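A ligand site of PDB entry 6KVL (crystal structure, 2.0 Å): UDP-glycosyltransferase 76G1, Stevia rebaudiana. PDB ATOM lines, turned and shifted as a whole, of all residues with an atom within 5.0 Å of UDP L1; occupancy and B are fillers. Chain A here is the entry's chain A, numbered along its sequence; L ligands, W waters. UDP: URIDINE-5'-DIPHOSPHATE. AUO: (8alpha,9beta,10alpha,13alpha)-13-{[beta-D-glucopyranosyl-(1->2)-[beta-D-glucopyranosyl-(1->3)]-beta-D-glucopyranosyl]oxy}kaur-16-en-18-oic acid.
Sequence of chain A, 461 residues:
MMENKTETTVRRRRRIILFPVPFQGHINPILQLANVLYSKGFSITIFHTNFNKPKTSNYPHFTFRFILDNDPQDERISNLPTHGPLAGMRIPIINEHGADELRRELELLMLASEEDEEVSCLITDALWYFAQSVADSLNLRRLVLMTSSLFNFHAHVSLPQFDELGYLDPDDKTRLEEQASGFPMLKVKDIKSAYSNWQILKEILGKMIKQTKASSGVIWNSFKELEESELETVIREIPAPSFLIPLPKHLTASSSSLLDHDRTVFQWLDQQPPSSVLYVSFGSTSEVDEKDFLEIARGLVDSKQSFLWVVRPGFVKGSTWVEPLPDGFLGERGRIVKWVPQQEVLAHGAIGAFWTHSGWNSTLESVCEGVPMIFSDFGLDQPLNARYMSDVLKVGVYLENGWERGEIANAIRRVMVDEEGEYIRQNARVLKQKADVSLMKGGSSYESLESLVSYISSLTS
O2 of AUO L2 sits at hydrogen-bond distance from O1B of UDP L1.
The backbone NH (N) of Ser 362 lies within hydrogen-bond range of an oxygen (O2A) of UDP L1, 3.0 Å away.
O3B of UDP L1 lies within hydrogen-bond range of OG of Ser 284, at 2.8 Å.
The side-chain hydroxyl of Ser 362 is in hydrogen-bond range of an oxygen (O2A) of UDP L1 (2.7 Å).
The backbone NH (N) of Asn 361 is in hydrogen-bond range of an oxygen (O1A) of UDP L1, 3.2 Å away.
N of Ser 284 sits at hydrogen-bond distance from O3B of UDP L1, at 2.7 Å.
The side-chain carboxylate (OE2) of Glu 365 is in hydrogen-bond range of an oxygen (O3') of UDP L1, 2.5 Å away.
NE2 of Gln 382 is in hydrogen-bond range of O3 of AUO L2 (3.0 Å).
An oxygen (O2') of UDP L1 sits close to the side-chain amide nitrogen of Gln 342, at 3.2 Å.
ND2 of Asn 28 sits at hydrogen-bond distance from O3' of UDP L1 (3.0 Å).
O1A of UDP L1 is in hydrogen-bond range of ND2 of Asn 361, at 2.9 Å.
An oxygen (O1B) of UDP L1 lies within hydrogen-bond range of a ring nitrogen (NE2) of His 357, at 2.8 Å.
The backbone NH (N) of Trp 360 sits at hydrogen-bond distance from an oxygen (O1A) of UDP L1 (3.5 Å).
An oxygen (O4) of UDP L1 lies within hydrogen-bond range of the backbone NH of Val 340 (3.1 Å).
The backbone NH (N) of Trp 360 sits at hydrogen-bond distance from an oxygen (O4) of AUO L2 (2.7 Å).
O of Val 340 lies within hydrogen-bond range of N3 of UDP L1.
OE1 of Gln 342 is in hydrogen-bond range of OH of Tyr 279, at 2.8 Å.
OG of Ser 362 is in hydrogen-bond range of NE2 of Gln 342, at 2.8 Å.
The side-chain carboxylate of Glu 365 sits at hydrogen-bond distance from the side-chain amide nitrogen of Gln 342, 2.9 Å away.
The side-chain amide oxygen (OD1) of Asn 28 is in hydrogen-bond range of the side-chain amide nitrogen (NE2) of Gln 24 (2.8 Å).
A ring nitrogen (ND1) of His 357 sits close to the backbone NH of Gly 359 (3.4 Å).
The backbone carbonyl oxygen of Gly 25 sits at hydrogen-bond distance from the side-chain amide nitrogen of Asn 361.
CG of Gln 24 touches O4' of UDP L1, 3.5 Å away.
CA of Gly 25 touches O2B of UDP L1, at 3.6 Å.
Tyr 279 touches UDP L1 (OH to O4, 3.6 Å).
Ser 281 touches UDP L1 (OG to C5, 3.8 Å).
Gly 283 touches UDP L1 (C to O3B, 3.6 Å).
Val 310 touches UDP L1 (CG1 to O4, 3.3 Å).
Trp 339 touches UDP L1.
Gly 359 touches UDP L1.
Water W5 lies within hydrogen-bond range of an oxygen (O2B) of UDP L1 (2.7 Å), an oxygen (O42) of AUO L2 (2.8 Å), the backbone NH (N) of Gly 25 (2.9 Å) and the side-chain hydroxyl (OG) of Ser 284 (3.5 Å).
Water W1 lies within hydrogen-bond range of O2 of UDP L1 and NE2 of His 261.
Water W2 lies within hydrogen-bond range of the backbone NH of Thr 285 (2.7 Å), an oxygen (O1B) of UDP L1 (2.8 Å) and the backbone NH of Ser 284 (3.4 Å).
Water W3 lies within hydrogen-bond range of an oxygen (O2') of UDP L1 (2.9 Å) and the backbone NH (N) of Gln 343 (3.0 Å).
Water W4 lies within hydrogen-bond range of the side-chain amide oxygen (OE1) of Gln 342 (2.7 Å), the side-chain hydroxyl (OG) of Ser 281 (2.8 Å) and the side-chain hydroxyl (OG) of Ser 362 (3.0 Å).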
ATOM      1  N   GLN A  24       1.157  -3.983  -2.477  1.00  0.00           N
ATOM      2  CA  GLN A  24      -0.294  -4.091  -2.659  1.00  0.00           C
ATOM      3  C   GLN A  24      -1.054  -3.990  -1.334  1.00  0.00           C
ATOM      4  O   GLN A  24      -2.078  -3.308  -1.254  1.00  0.00           O
ATOM      5  CB  GLN A  24      -0.630  -5.414  -3.346  1.00  0.00           C
ATOM      6  CG  GLN A  24      -2.085  -5.492  -3.831  1.00  0.00           C
ATOM      7  CD  GLN A  24      -2.321  -4.597  -5.034  1.00  0.00           C
ATOM      8  OE1 GLN A  24      -2.068  -4.994  -6.173  1.00  0.00           O
ATOM      9  NE2 GLN A  24      -2.819  -3.389  -4.800  1.00  0.00           N
ATOM     10  N   GLY A  25      -0.572  -4.684  -0.297  1.00  0.00           N
ATOM     11  CA  GLY A  25      -1.191  -4.662   1.012  1.00  0.00           C
ATOM     12  C   GLY A  25      -1.073  -3.359   1.755  1.00  0.00           C
ATOM     13  O   GLY A  25      -1.663  -3.189   2.830  1.00  0.00           O
ATOM     14  N   ASN A  28      -3.307  -0.431  -0.999  1.00  0.00           N
ATOM     15  CA  ASN A  28      -4.769  -0.611  -0.964  1.00  0.00           C
ATOM     16  C   ASN A  28      -5.406   0.153   0.192  1.00  0.00           C
ATOM     17  O   ASN A  28      -6.248   1.030  -0.061  1.00  0.00           O
ATOM     18  CB  ASN A  28      -5.110  -2.100  -0.933  1.00  0.00           C
ATOM     19  CG  ASN A  28      -5.073  -2.731  -2.315  1.00  0.00           C
ATOM     20  OD1 ASN A  28      -4.749  -2.065  -3.290  1.00  0.00           O
ATOM     21  ND2 ASN A  28      -5.407  -4.006  -2.407  1.00  0.00           N
ATOM     22  N   ALA A 253     -10.779  -2.019  -2.904  1.00  0.00           N
ATOM     23  CA  ALA A 253      -9.510  -1.486  -3.356  1.00  0.00           C
ATOM     24  C   ALA A 253      -9.253  -1.765  -4.833  1.00  0.00           C
ATOM     25  O   ALA A 253      -8.093  -1.795  -5.272  1.00  0.00           O
ATOM     26  CB  ALA A 253      -8.368  -2.063  -2.508  1.00  0.00           C
ATOM     27  N   HIS A 261      -6.923  -7.268 -13.697  1.00  0.00           N
ATOM     28  CA  HIS A 261      -7.968  -8.175 -13.238  1.00  0.00           C
ATOM     29  C   HIS A 261      -8.342  -9.161 -14.342  1.00  0.00           C
ATOM     30  O   HIS A 261      -8.498  -8.788 -15.504  1.00  0.00           O
ATOM     31  CB  HIS A 261      -9.217  -7.390 -12.830  1.00  0.00           C
ATOM     32  CG  HIS A 261      -9.042  -6.560 -11.605  1.00  0.00           C
ATOM     33  ND1 HIS A 261      -9.541  -5.283 -11.494  1.00  0.00           N
ATOM     34  CD2 HIS A 261      -8.401  -6.810 -10.441  1.00  0.00           C
ATOM     35  CE1 HIS A 261      -9.221  -4.785 -10.312  1.00  0.00           C
ATOM     36  NE2 HIS A 261      -8.524  -5.682  -9.655  1.00  0.00           N
ATOM     37  N   TYR A 279     -12.868 -19.788  -2.596  1.00  0.00           N
ATOM     38  CA  TYR A 279     -11.909 -18.852  -3.161  1.00  0.00           C
ATOM     39  C   TYR A 279     -10.562 -19.082  -2.489  1.00  0.00           C
ATOM     40  O   TYR A 279     -10.484 -19.215  -1.260  1.00  0.00           O
ATOM     41  CB  TYR A 279     -12.384 -17.402  -2.962  1.00  0.00           C
ATOM     42  CG  TYR A 279     -11.376 -16.367  -3.416  1.00  0.00           C
ATOM     43  CD1 TYR A 279     -11.067 -16.209  -4.764  1.00  0.00           C
ATOM     44  CD2 TYR A 279     -10.736 -15.547  -2.501  1.00  0.00           C
ATOM     45  CE1 TYR A 279     -10.137 -15.258  -5.180  1.00  0.00           C
ATOM     46  CE2 TYR A 279      -9.807 -14.621  -2.902  1.00  0.00           C
ATOM     47  CZ  TYR A 279      -9.515 -14.464  -4.246  1.00  0.00           C
ATOM     48  OH  TYR A 279      -8.590 -13.500  -4.633  1.00  0.00           O
ATOM     49  N   SER A 281      -6.437 -17.869  -2.363  1.00  0.00           N
ATOM     50  CA  SER A 281      -5.415 -16.904  -2.743  1.00  0.00           C
ATOM     51  C   SER A 281      -4.429 -16.784  -1.592  1.00  0.00           C
ATOM     52  O   SER A 281      -4.828 -16.515  -0.457  1.00  0.00           O
ATOM     53  CB  SER A 281      -6.018 -15.554  -3.072  1.00  0.00           C
ATOM     54  OG  SER A 281      -4.990 -14.603  -3.282  1.00  0.00           O
ATOM     55  N   GLY A 283      -1.859 -14.602  -1.349  1.00  0.00           N
ATOM     56  CA  GLY A 283      -1.330 -13.267  -1.111  1.00  0.00           C
ATOM     57  C   GLY A 283      -0.676 -12.668  -2.343  1.00  0.00           C
ATOM     58  O   GLY A 283      -0.848 -13.146  -3.479  1.00  0.00           O
ATOM     59  N   SER A 284       0.075 -11.588  -2.122  1.00  0.00           N
ATOM     60  CA  SER A 284       0.750 -10.922  -3.215  1.00  0.00           C
ATOM     61  C   SER A 284       2.266 -11.092  -3.208  1.00  0.00           C
ATOM     62  O   SER A 284       2.918 -10.620  -4.144  1.00  0.00           O
ATOM     63  CB  SER A 284       0.366  -9.433  -3.270  1.00  0.00           C
ATOM     64  OG  SER A 284       0.980  -8.658  -2.249  1.00  0.00           O
ATOM     65  N   THR A 285       2.862 -11.803  -2.220  1.00  0.00           N
ATOM     66  CA  THR A 285       4.294 -12.077  -2.294  1.00  0.00           C
ATOM     67  C   THR A 285       4.744 -13.454  -1.837  1.00  0.00           C
ATOM     68  O   THR A 285       5.946 -13.729  -1.907  1.00  0.00           O
ATOM     69  CB  THR A 285       5.106 -11.020  -1.484  1.00  0.00           C
ATOM     70  OG1 THR A 285       5.245 -11.432  -0.124  1.00  0.00           O
ATOM     71  CG2 THR A 285       4.449  -9.641  -1.522  1.00  0.00           C
ATOM     72  N   VAL A 310      -6.531 -18.120  -7.212  1.00  0.00           N
ATOM     73  CA  VAL A 310      -5.603 -17.106  -7.706  1.00  0.00           C
ATOM     74  C   VAL A 310      -4.180 -17.593  -7.450  1.00  0.00           C
ATOM     75  O   VAL A 310      -3.763 -17.759  -6.294  1.00  0.00           O
ATOM     76  CB  VAL A 310      -5.838 -15.750  -7.040  1.00  0.00           C
ATOM     77  CG1 VAL A 310      -4.770 -14.747  -7.496  1.00  0.00           C
ATOM     78  CG2 VAL A 310      -7.239 -15.209  -7.353  1.00  0.00           C
ATOM     79  N   LYS A 338      -4.746 -15.607 -12.526  1.00  0.00           N
ATOM     80  CA  LYS A 338      -3.595 -14.852 -12.059  1.00  0.00           C
ATOM     81  C   LYS A 338      -3.965 -13.780 -11.046  1.00  0.00           C
ATOM     82  O   LYS A 338      -3.162 -13.471 -10.170  1.00  0.00           O
ATOM     83  CB  LYS A 338      -2.881 -14.179 -13.236  1.00  0.00           C
ATOM     84  CG  LYS A 338      -2.265 -15.147 -14.255  1.00  0.00           C
ATOM     85  CD  LYS A 338      -1.557 -14.376 -15.376  1.00  0.00           C
ATOM     86  CE  LYS A 338      -1.254 -15.259 -16.571  1.00  0.00           C
ATOM     87  NZ  LYS A 338      -0.524 -16.478 -16.148  1.00  0.00           N
ATOM     88  N   TRP A 339      -5.167 -13.216 -11.150  1.00  0.00           N
ATOM     89  CA  TRP A 339      -5.502 -12.042 -10.349  1.00  0.00           C
ATOM     90  C   TRP A 339      -6.955 -11.689 -10.572  1.00  0.00           C
ATOM     91  O   TRP A 339      -7.441 -11.763 -11.712  1.00  0.00           O
ATOM     92  CB  TRP A 339      -4.607 -10.865 -10.744  1.00  0.00           C
ATOM     93  CG  TRP A 339      -4.556  -9.769  -9.760  1.00  0.00           C
ATOM     94  CD1 TRP A 339      -5.063  -8.516  -9.899  1.00  0.00           C
ATOM     95  CD2 TRP A 339      -3.915  -9.806  -8.481  1.00  0.00           C
ATOM     96  NE1 TRP A 339      -4.777  -7.768  -8.789  1.00  0.00           N
ATOM     97  CE2 TRP A 339      -4.080  -8.543  -7.901  1.00  0.00           C
ATOM     98  CE3 TRP A 339      -3.222 -10.794  -7.775  1.00  0.00           C
ATOM     99  CZ2 TRP A 339      -3.593  -8.233  -6.639  1.00  0.00           C
ATOM    100  CZ3 TRP A 339      -2.732 -10.486  -6.523  1.00  0.00           C
ATOM    101  CH2 TRP A 339      -2.920  -9.215  -5.965  1.00  0.00           C
ATOM    102  N   VAL A 340      -7.655 -11.283  -9.508  1.00  0.00           N
ATOM    103  CA  VAL A 340      -9.066 -10.914  -9.607  1.00  0.00           C
ATOM    104  C   VAL A 340      -9.318  -9.639  -8.802  1.00  0.00           C
ATOM    105  O   VAL A 340      -8.449  -9.202  -8.031  1.00  0.00           O
ATOM    106  CB  VAL A 340      -9.961 -12.058  -9.087  1.00  0.00           C
ATOM    107  CG1 VAL A 340      -9.732 -13.328  -9.892  1.00  0.00           C
ATOM    108  CG2 VAL A 340      -9.696 -12.293  -7.587  1.00  0.00           C
ATOM    109  N   PRO A 341     -10.471  -9.020  -8.938  1.00  0.00           N
ATOM    110  CA  PRO A 341     -10.874  -8.021  -7.948  1.00  0.00           C
ATOM    111  C   PRO A 341     -11.313  -8.774  -6.698  1.00  0.00           C
ATOM    112  O   PRO A 341     -12.450  -9.267  -6.648  1.00  0.00           O
ATOM    113  CB  PRO A 341     -12.040  -7.284  -8.616  1.00  0.00           C
ATOM    114  CG  PRO A 341     -12.074  -7.789 -10.062  1.00  0.00           C
ATOM    115  CD  PRO A 341     -11.459  -9.148 -10.023  1.00  0.00           C
ATOM    116  N   GLN A 342     -10.422  -8.900  -5.717  1.00  0.00           N
ATOM    117  CA  GLN A 342     -10.630  -9.915  -4.687  1.00  0.00           C
ATOM    118  C   GLN A 342     -11.879  -9.665  -3.864  1.00  0.00           C
ATOM    119  O   GLN A 342     -12.674 -10.591  -3.650  1.00  0.00           O
ATOM    120  CB  GLN A 342      -9.419 -10.013  -3.754  1.00  0.00           C
ATOM    121  CG  GLN A 342      -9.730 -10.848  -2.525  1.00  0.00           C
ATOM    122  CD  GLN A 342      -8.485 -11.336  -1.804  1.00  0.00           C
ATOM    123  OE1 GLN A 342      -7.710 -12.133  -2.349  1.00  0.00           O
ATOM    124  NE2 GLN A 342      -8.294 -10.872  -0.571  1.00  0.00           N
ATOM    125  N   GLN A 343     -12.061  -8.444  -3.338  1.00  0.00           N
ATOM    126  CA  GLN A 343     -13.216  -8.222  -2.472  1.00  0.00           C
ATOM    127  C   GLN A 343     -14.517  -8.393  -3.239  1.00  0.00           C
ATOM    128  O   GLN A 343     -15.496  -8.941  -2.719  1.00  0.00           O
ATOM    129  CB  GLN A 343     -13.158  -6.837  -1.801  1.00  0.00           C
ATOM    130  CG  GLN A 343     -14.301  -6.661  -0.746  1.00  0.00           C
ATOM    131  CD  GLN A 343     -14.246  -5.323   0.010  1.00  0.00           C
ATOM    132  OE1 GLN A 343     -13.242  -4.607  -0.004  1.00  0.00           O
ATOM    133  NE2 GLN A 343     -15.348  -5.000   0.682  1.00  0.00           N
ATOM    134  N   HIS A 357      -3.934 -16.762   2.959  1.00  0.00           N
ATOM    135  CA  HIS A 357      -2.673 -16.770   3.687  1.00  0.00           C
ATOM    136  C   HIS A 357      -2.715 -15.918   4.951  1.00  0.00           C
ATOM    137  O   HIS A 357      -1.710 -15.814   5.641  1.00  0.00           O
ATOM    138  CB  HIS A 357      -1.518 -16.281   2.790  1.00  0.00           C
ATOM    139  CG  HIS A 357      -1.460 -14.795   2.599  1.00  0.00           C
ATOM    140  ND1 HIS A 357      -2.536 -14.055   2.154  1.00  0.00           N
ATOM    141  CD2 HIS A 357      -0.437 -13.913   2.750  1.00  0.00           C
ATOM    142  CE1 HIS A 357      -2.190 -12.776   2.053  1.00  0.00           C
ATOM    143  NE2 HIS A 357      -0.918 -12.669   2.425  1.00  0.00           N
ATOM    144  N   GLY A 359      -3.069 -12.608   5.202  1.00  0.00           N
ATOM    145  CA  GLY A 359      -2.744 -11.202   5.124  1.00  0.00           C
ATOM    146  C   GLY A 359      -3.866 -10.402   5.735  1.00  0.00           C
ATOM    147  O   GLY A 359      -5.024 -10.839   5.678  1.00  0.00           O
ATOM    148  N   TRP A 360      -3.573  -9.225   6.332  1.00  0.00           N
ATOM    149  CA  TRP A 360      -4.630  -8.529   7.076  1.00  0.00           C
ATOM    150  C   TRP A 360      -5.719  -7.993   6.148  1.00  0.00           C
ATOM    151  O   TRP A 360      -6.910  -8.077   6.474  1.00  0.00           O
ATOM    152  CB  TRP A 360      -4.060  -7.394   7.926  1.00  0.00           C
ATOM    153  CG  TRP A 360      -5.125  -6.716   8.758  1.00  0.00           C
ATOM    154  CD1 TRP A 360      -5.550  -5.419   8.665  1.00  0.00           C
ATOM    155  CD2 TRP A 360      -5.910  -7.329   9.796  1.00  0.00           C
ATOM    156  NE1 TRP A 360      -6.553  -5.181   9.591  1.00  0.00           N
ATOM    157  CE2 TRP A 360      -6.797  -6.339  10.294  1.00  0.00           C
ATOM    158  CE3 TRP A 360      -5.959  -8.605  10.359  1.00  0.00           C
ATOM    159  CZ2 TRP A 360      -7.713  -6.597  11.312  1.00  0.00           C
ATOM    160  CZ3 TRP A 360      -6.863  -8.860  11.382  1.00  0.00           C
ATOM    161  CH2 TRP A 360      -7.729  -7.855  11.841  1.00  0.00           C
ATOM    162  N   ASN A 361      -5.337  -7.436   4.986  1.00  0.00           N
ATOM    163  CA  ASN A 361      -6.353  -6.931   4.060  1.00  0.00           C
ATOM    164  C   ASN A 361      -7.296  -8.037   3.611  1.00  0.00           C
ATOM    165  O   ASN A 361      -8.511  -7.854   3.594  1.00  0.00           O
ATOM    166  CB  ASN A 361      -5.692  -6.287   2.834  1.00  0.00           C
ATOM    167  CG  ASN A 361      -4.942  -5.048   3.191  1.00  0.00           C
ATOM    168  OD1 ASN A 361      -5.545  -3.988   3.441  1.00  0.00           O
ATOM    169  ND2 ASN A 361      -3.614  -5.160   3.264  1.00  0.00           N
ATOM    170  N   SER A 362      -6.744  -9.190   3.214  1.00  0.00           N
ATOM    171  CA  SER A 362      -7.607 -10.297   2.797  1.00  0.00           C
ATOM    172  C   SER A 362      -8.478 -10.760   3.959  1.00  0.00           C
ATOM    173  O   SER A 362      -9.675 -11.038   3.781  1.00  0.00           O
ATOM    174  CB  SER A 362      -6.778 -11.479   2.267  1.00  0.00           C
ATOM    175  OG  SER A 362      -6.023 -11.119   1.109  1.00  0.00           O
ATOM    176  N   GLU A 365     -11.184  -8.076   4.531  1.00  0.00           N
ATOM    177  CA  GLU A 365     -12.136  -8.101   3.410  1.00  0.00           C
ATOM    178  C   GLU A 365     -13.112  -9.261   3.570  1.00  0.00           C
ATOM    179  O   GLU A 365     -14.322  -9.106   3.352  1.00  0.00           O
ATOM    180  CB  GLU A 365     -11.371  -8.218   2.079  1.00  0.00           C
ATOM    181  CG  GLU A 365     -10.582  -6.939   1.721  1.00  0.00           C
ATOM    182  CD  GLU A 365      -9.453  -7.175   0.726  1.00  0.00           C
ATOM    183  OE1 GLU A 365      -9.385  -8.258   0.106  1.00  0.00           O
ATOM    184  OE2 GLU A 365      -8.611  -6.268   0.579  1.00  0.00           O
ATOM    185  N   GLN A 382       0.806 -12.827   9.674  1.00  0.00           N
ATOM    186  CA  GLN A 382      -0.195 -13.787   9.218  1.00  0.00           C
ATOM    187  C   GLN A 382      -0.540 -14.872  10.237  1.00  0.00           C
ATOM    188  O   GLN A 382      -1.731 -15.151  10.424  1.00  0.00           O
ATOM    189  CB  GLN A 382       0.287 -14.383   7.879  1.00  0.00           C
ATOM    190  CG  GLN A 382       0.451 -13.268   6.823  1.00  0.00           C
ATOM    191  CD  GLN A 382       1.389 -13.617   5.672  1.00  0.00           C
ATOM    192  OE1 GLN A 382       1.631 -14.789   5.392  1.00  0.00           O
ATOM    193  NE2 GLN A 382       1.894 -12.599   5.003  1.00  0.00           N
HETATM  194  N1  UDP L   1      -5.865  -8.991  -4.058  1.00  0.00           N
HETATM  195  C2  UDP L   1      -6.570  -8.762  -5.266  1.00  0.00           C
HETATM  196  N3  UDP L   1      -6.661  -9.690  -6.232  1.00  0.00           N
HETATM  197  C4  UDP L   1      -6.098 -10.920  -6.007  1.00  0.00           C
HETATM  198  C5  UDP L   1      -5.414 -11.148  -4.786  1.00  0.00           C
HETATM  199  C6  UDP L   1      -5.311 -10.171  -3.869  1.00  0.00           C
HETATM  200  O2  UDP L   1      -7.029  -7.630  -5.343  1.00  0.00           O
HETATM  201  O4  UDP L   1      -6.185 -11.870  -6.835  1.00  0.00           O
HETATM  202  C1' UDP L   1      -5.718  -7.936  -3.028  1.00  0.00           C
HETATM  203  C2' UDP L   1      -6.534  -8.200  -1.769  1.00  0.00           C
HETATM  204  O2' UDP L   1      -7.890  -7.989  -1.948  1.00  0.00           O
HETATM  205  C3' UDP L   1      -5.803  -7.353  -0.724  1.00  0.00           C
HETATM  206  C4' UDP L   1      -4.326  -7.422  -1.255  1.00  0.00           C
HETATM  207  O4' UDP L   1      -4.415  -7.822  -2.600  1.00  0.00           O
HETATM  208  O3' UDP L   1      -6.357  -6.094  -0.544  1.00  0.00           O
HETATM  209  C5' UDP L   1      -3.400  -8.349  -0.443  1.00  0.00           C
HETATM  210  O5' UDP L   1      -3.176  -7.907   0.851  1.00  0.00           O
HETATM  211  PA  UDP L   1      -2.919  -8.785   2.092  1.00  0.00           P
HETATM  212  O1A UDP L   1      -2.801  -7.944   3.183  1.00  0.00           O
HETATM  213  O2A UDP L   1      -3.950  -9.747   2.216  1.00  0.00           O
HETATM  214  O3A UDP L   1      -1.669  -9.691   1.828  1.00  0.00           O
HETATM  215  PB  UDP L   1      -0.278  -9.460   1.140  1.00  0.00           P
HETATM  216  O1B UDP L   1       0.551 -10.315   1.877  1.00  0.00           O
HETATM  217  O2B UDP L   1      -0.014  -8.107   1.244  1.00  0.00           O
HETATM  218  O3B UDP L   1      -0.564  -9.826  -0.183  1.00  0.00           O
HETATM  219  O6  AUO L   2       0.182  -4.793   6.730  1.00  0.00           O
HETATM  220  C6  AUO L   2      -0.644  -5.273   5.743  1.00  0.00           C
HETATM  221  C5  AUO L   2      -0.103  -6.515   5.029  1.00  0.00           C
HETATM  222  C4  AUO L   2       0.065  -7.681   6.001  1.00  0.00           C
HETATM  223  O4  AUO L   2      -1.107  -8.068   6.598  1.00  0.00           O
HETATM  224  C3  AUO L   2       0.733  -8.881   5.200  1.00  0.00           C
HETATM  225  O3  AUO L   2       0.933  -9.955   6.047  1.00  0.00           O
HETATM  226  O5  AUO L   2       1.123  -6.204   4.501  1.00  0.00           O
HETATM  227  C1  AUO L   2       1.818  -7.105   3.766  1.00  0.00           C
HETATM  228  C2  AUO L   2       2.078  -8.430   4.541  1.00  0.00           C
HETATM  229  O2  AUO L   2       2.602  -9.436   3.678  1.00  0.00           O
HETATM  230  O61 AUO L   2       6.403  -7.624  11.401  1.00  0.00           O
HETATM  231  C61 AUO L   2       6.246  -7.921  10.053  1.00  0.00           C
HETATM  232  C51 AUO L   2       5.614  -6.758   9.297  1.00  0.00           C
HETATM  233  C41 AUO L   2       4.249  -6.372   9.949  1.00  0.00           C
HETATM  234  O41 AUO L   2       4.378  -5.961  11.265  1.00  0.00           O
HETATM  235  C31 AUO L   2       3.528  -5.285   9.137  1.00  0.00           C
HETATM  236  O31 AUO L   2       2.304  -4.923   9.731  1.00  0.00           O
HETATM  237  O51 AUO L   2       5.404  -7.063   7.929  1.00  0.00           O
HETATM  238  C11 AUO L   2       4.775  -6.141   7.163  1.00  0.00           C
HETATM  239  C21 AUO L   2       3.370  -5.802   7.741  1.00  0.00           C
HETATM  240  O21 AUO L   2       2.720  -4.895   6.915  1.00  0.00           O
HETATM  241  O62 AUO L   2       8.328  -7.376   0.680  1.00  0.00           O
HETATM  242  C64 AUO L   2       7.106  -6.667   0.828  1.00  0.00           C
HETATM  243  C52 AUO L   2       6.428  -6.938   2.210  1.00  0.00           C
HETATM  244  C42 AUO L   2       4.974  -6.519   2.161  1.00  0.00           C
HETATM  245  O42 AUO L   2       4.329  -7.082   1.056  1.00  0.00           O
HETATM  246  C32 AUO L   2       4.281  -6.887   3.500  1.00  0.00           C
HETATM  247  O32 AUO L   2       2.943  -6.368   3.470  1.00  0.00           O
HETATM  248  O52 AUO L   2       7.059  -6.235   3.295  1.00  0.00           O
HETATM  249  C62 AUO L   2       6.621  -6.605   4.608  1.00  0.00           C
HETATM  250  C19 AUO L   2       8.495  -4.754   7.738  1.00  0.00           C
HETATM  251  C22 AUO L   2       5.090  -6.271   4.696  1.00  0.00           C
HETATM  252  O22 AUO L   2       4.612  -6.776   5.929  1.00  0.00           O
HETATM  253  O11 AUO L   2      12.637  -8.460   1.431  1.00  0.00           O
HETATM  254  C55 AUO L   2      12.974  -9.428   2.118  1.00  0.00           C
HETATM  255  O   AUO L   2      12.846 -10.585   1.760  1.00  0.00           O
HETATM  256  C23 AUO L   2      13.764  -9.149   3.400  1.00  0.00           C
HETATM  257  C15 AUO L   2      14.108 -10.451   4.184  1.00  0.00           C
HETATM  258  C54 AUO L   2      15.086  -8.512   2.907  1.00  0.00           C
HETATM  259  C53 AUO L   2      13.060  -8.200   4.397  1.00  0.00           C
HETATM  260  C63 AUO L   2      12.615  -6.898   3.715  1.00  0.00           C
HETATM  261  C7  AUO L   2      12.198  -5.856   4.746  1.00  0.00           C
HETATM  262  C9  AUO L   2      11.010  -6.338   5.584  1.00  0.00           C
HETATM  263  C17 AUO L   2      10.640  -5.363   6.757  1.00  0.00           C
HETATM  264  C14 AUO L   2       9.249  -5.511   6.914  1.00  0.00           C
HETATM  265  C10 AUO L   2       9.696  -6.255   4.788  1.00  0.00           C
HETATM  266  C18 AUO L   2       8.731  -6.379   5.938  1.00  0.00           C
HETATM  267  C12 AUO L   2       8.698  -7.835   6.430  1.00  0.00           C
HETATM  268  C13 AUO L   2      10.025  -8.292   6.927  1.00  0.00           C
HETATM  269  C8  AUO L   2      11.278  -7.779   6.143  1.00  0.00           C
HETATM  270  C43 AUO L   2      11.838  -8.828   5.105  1.00  0.00           C
HETATM  271  C16 AUO L   2      10.772  -9.219   4.069  1.00  0.00           C
HETATM  272  C33 AUO L   2      12.286 -10.078   5.856  1.00  0.00           C
HETATM  273  C   AUO L   2      12.949 -11.044   4.933  1.00  0.00           C
HETATM  274  O19 AUO L   2       7.389  -5.942   5.592  1.00  0.00           O
HETATM  275  O   HOH W   1      -8.113  -5.634  -6.831  1.00  0.00           O
HETATM  276  O   HOH W   2       2.283 -11.912   0.412  1.00  0.00           O
HETATM  277  O   HOH W   3      -9.992  -6.358  -3.031  1.00  0.00           O
HETATM  278  O   HOH W   4      -5.179 -12.542  -1.421  1.00  0.00           O
HETATM  279  O   HOH W   5       1.730  -6.321   0.244  1.00  0.00           O
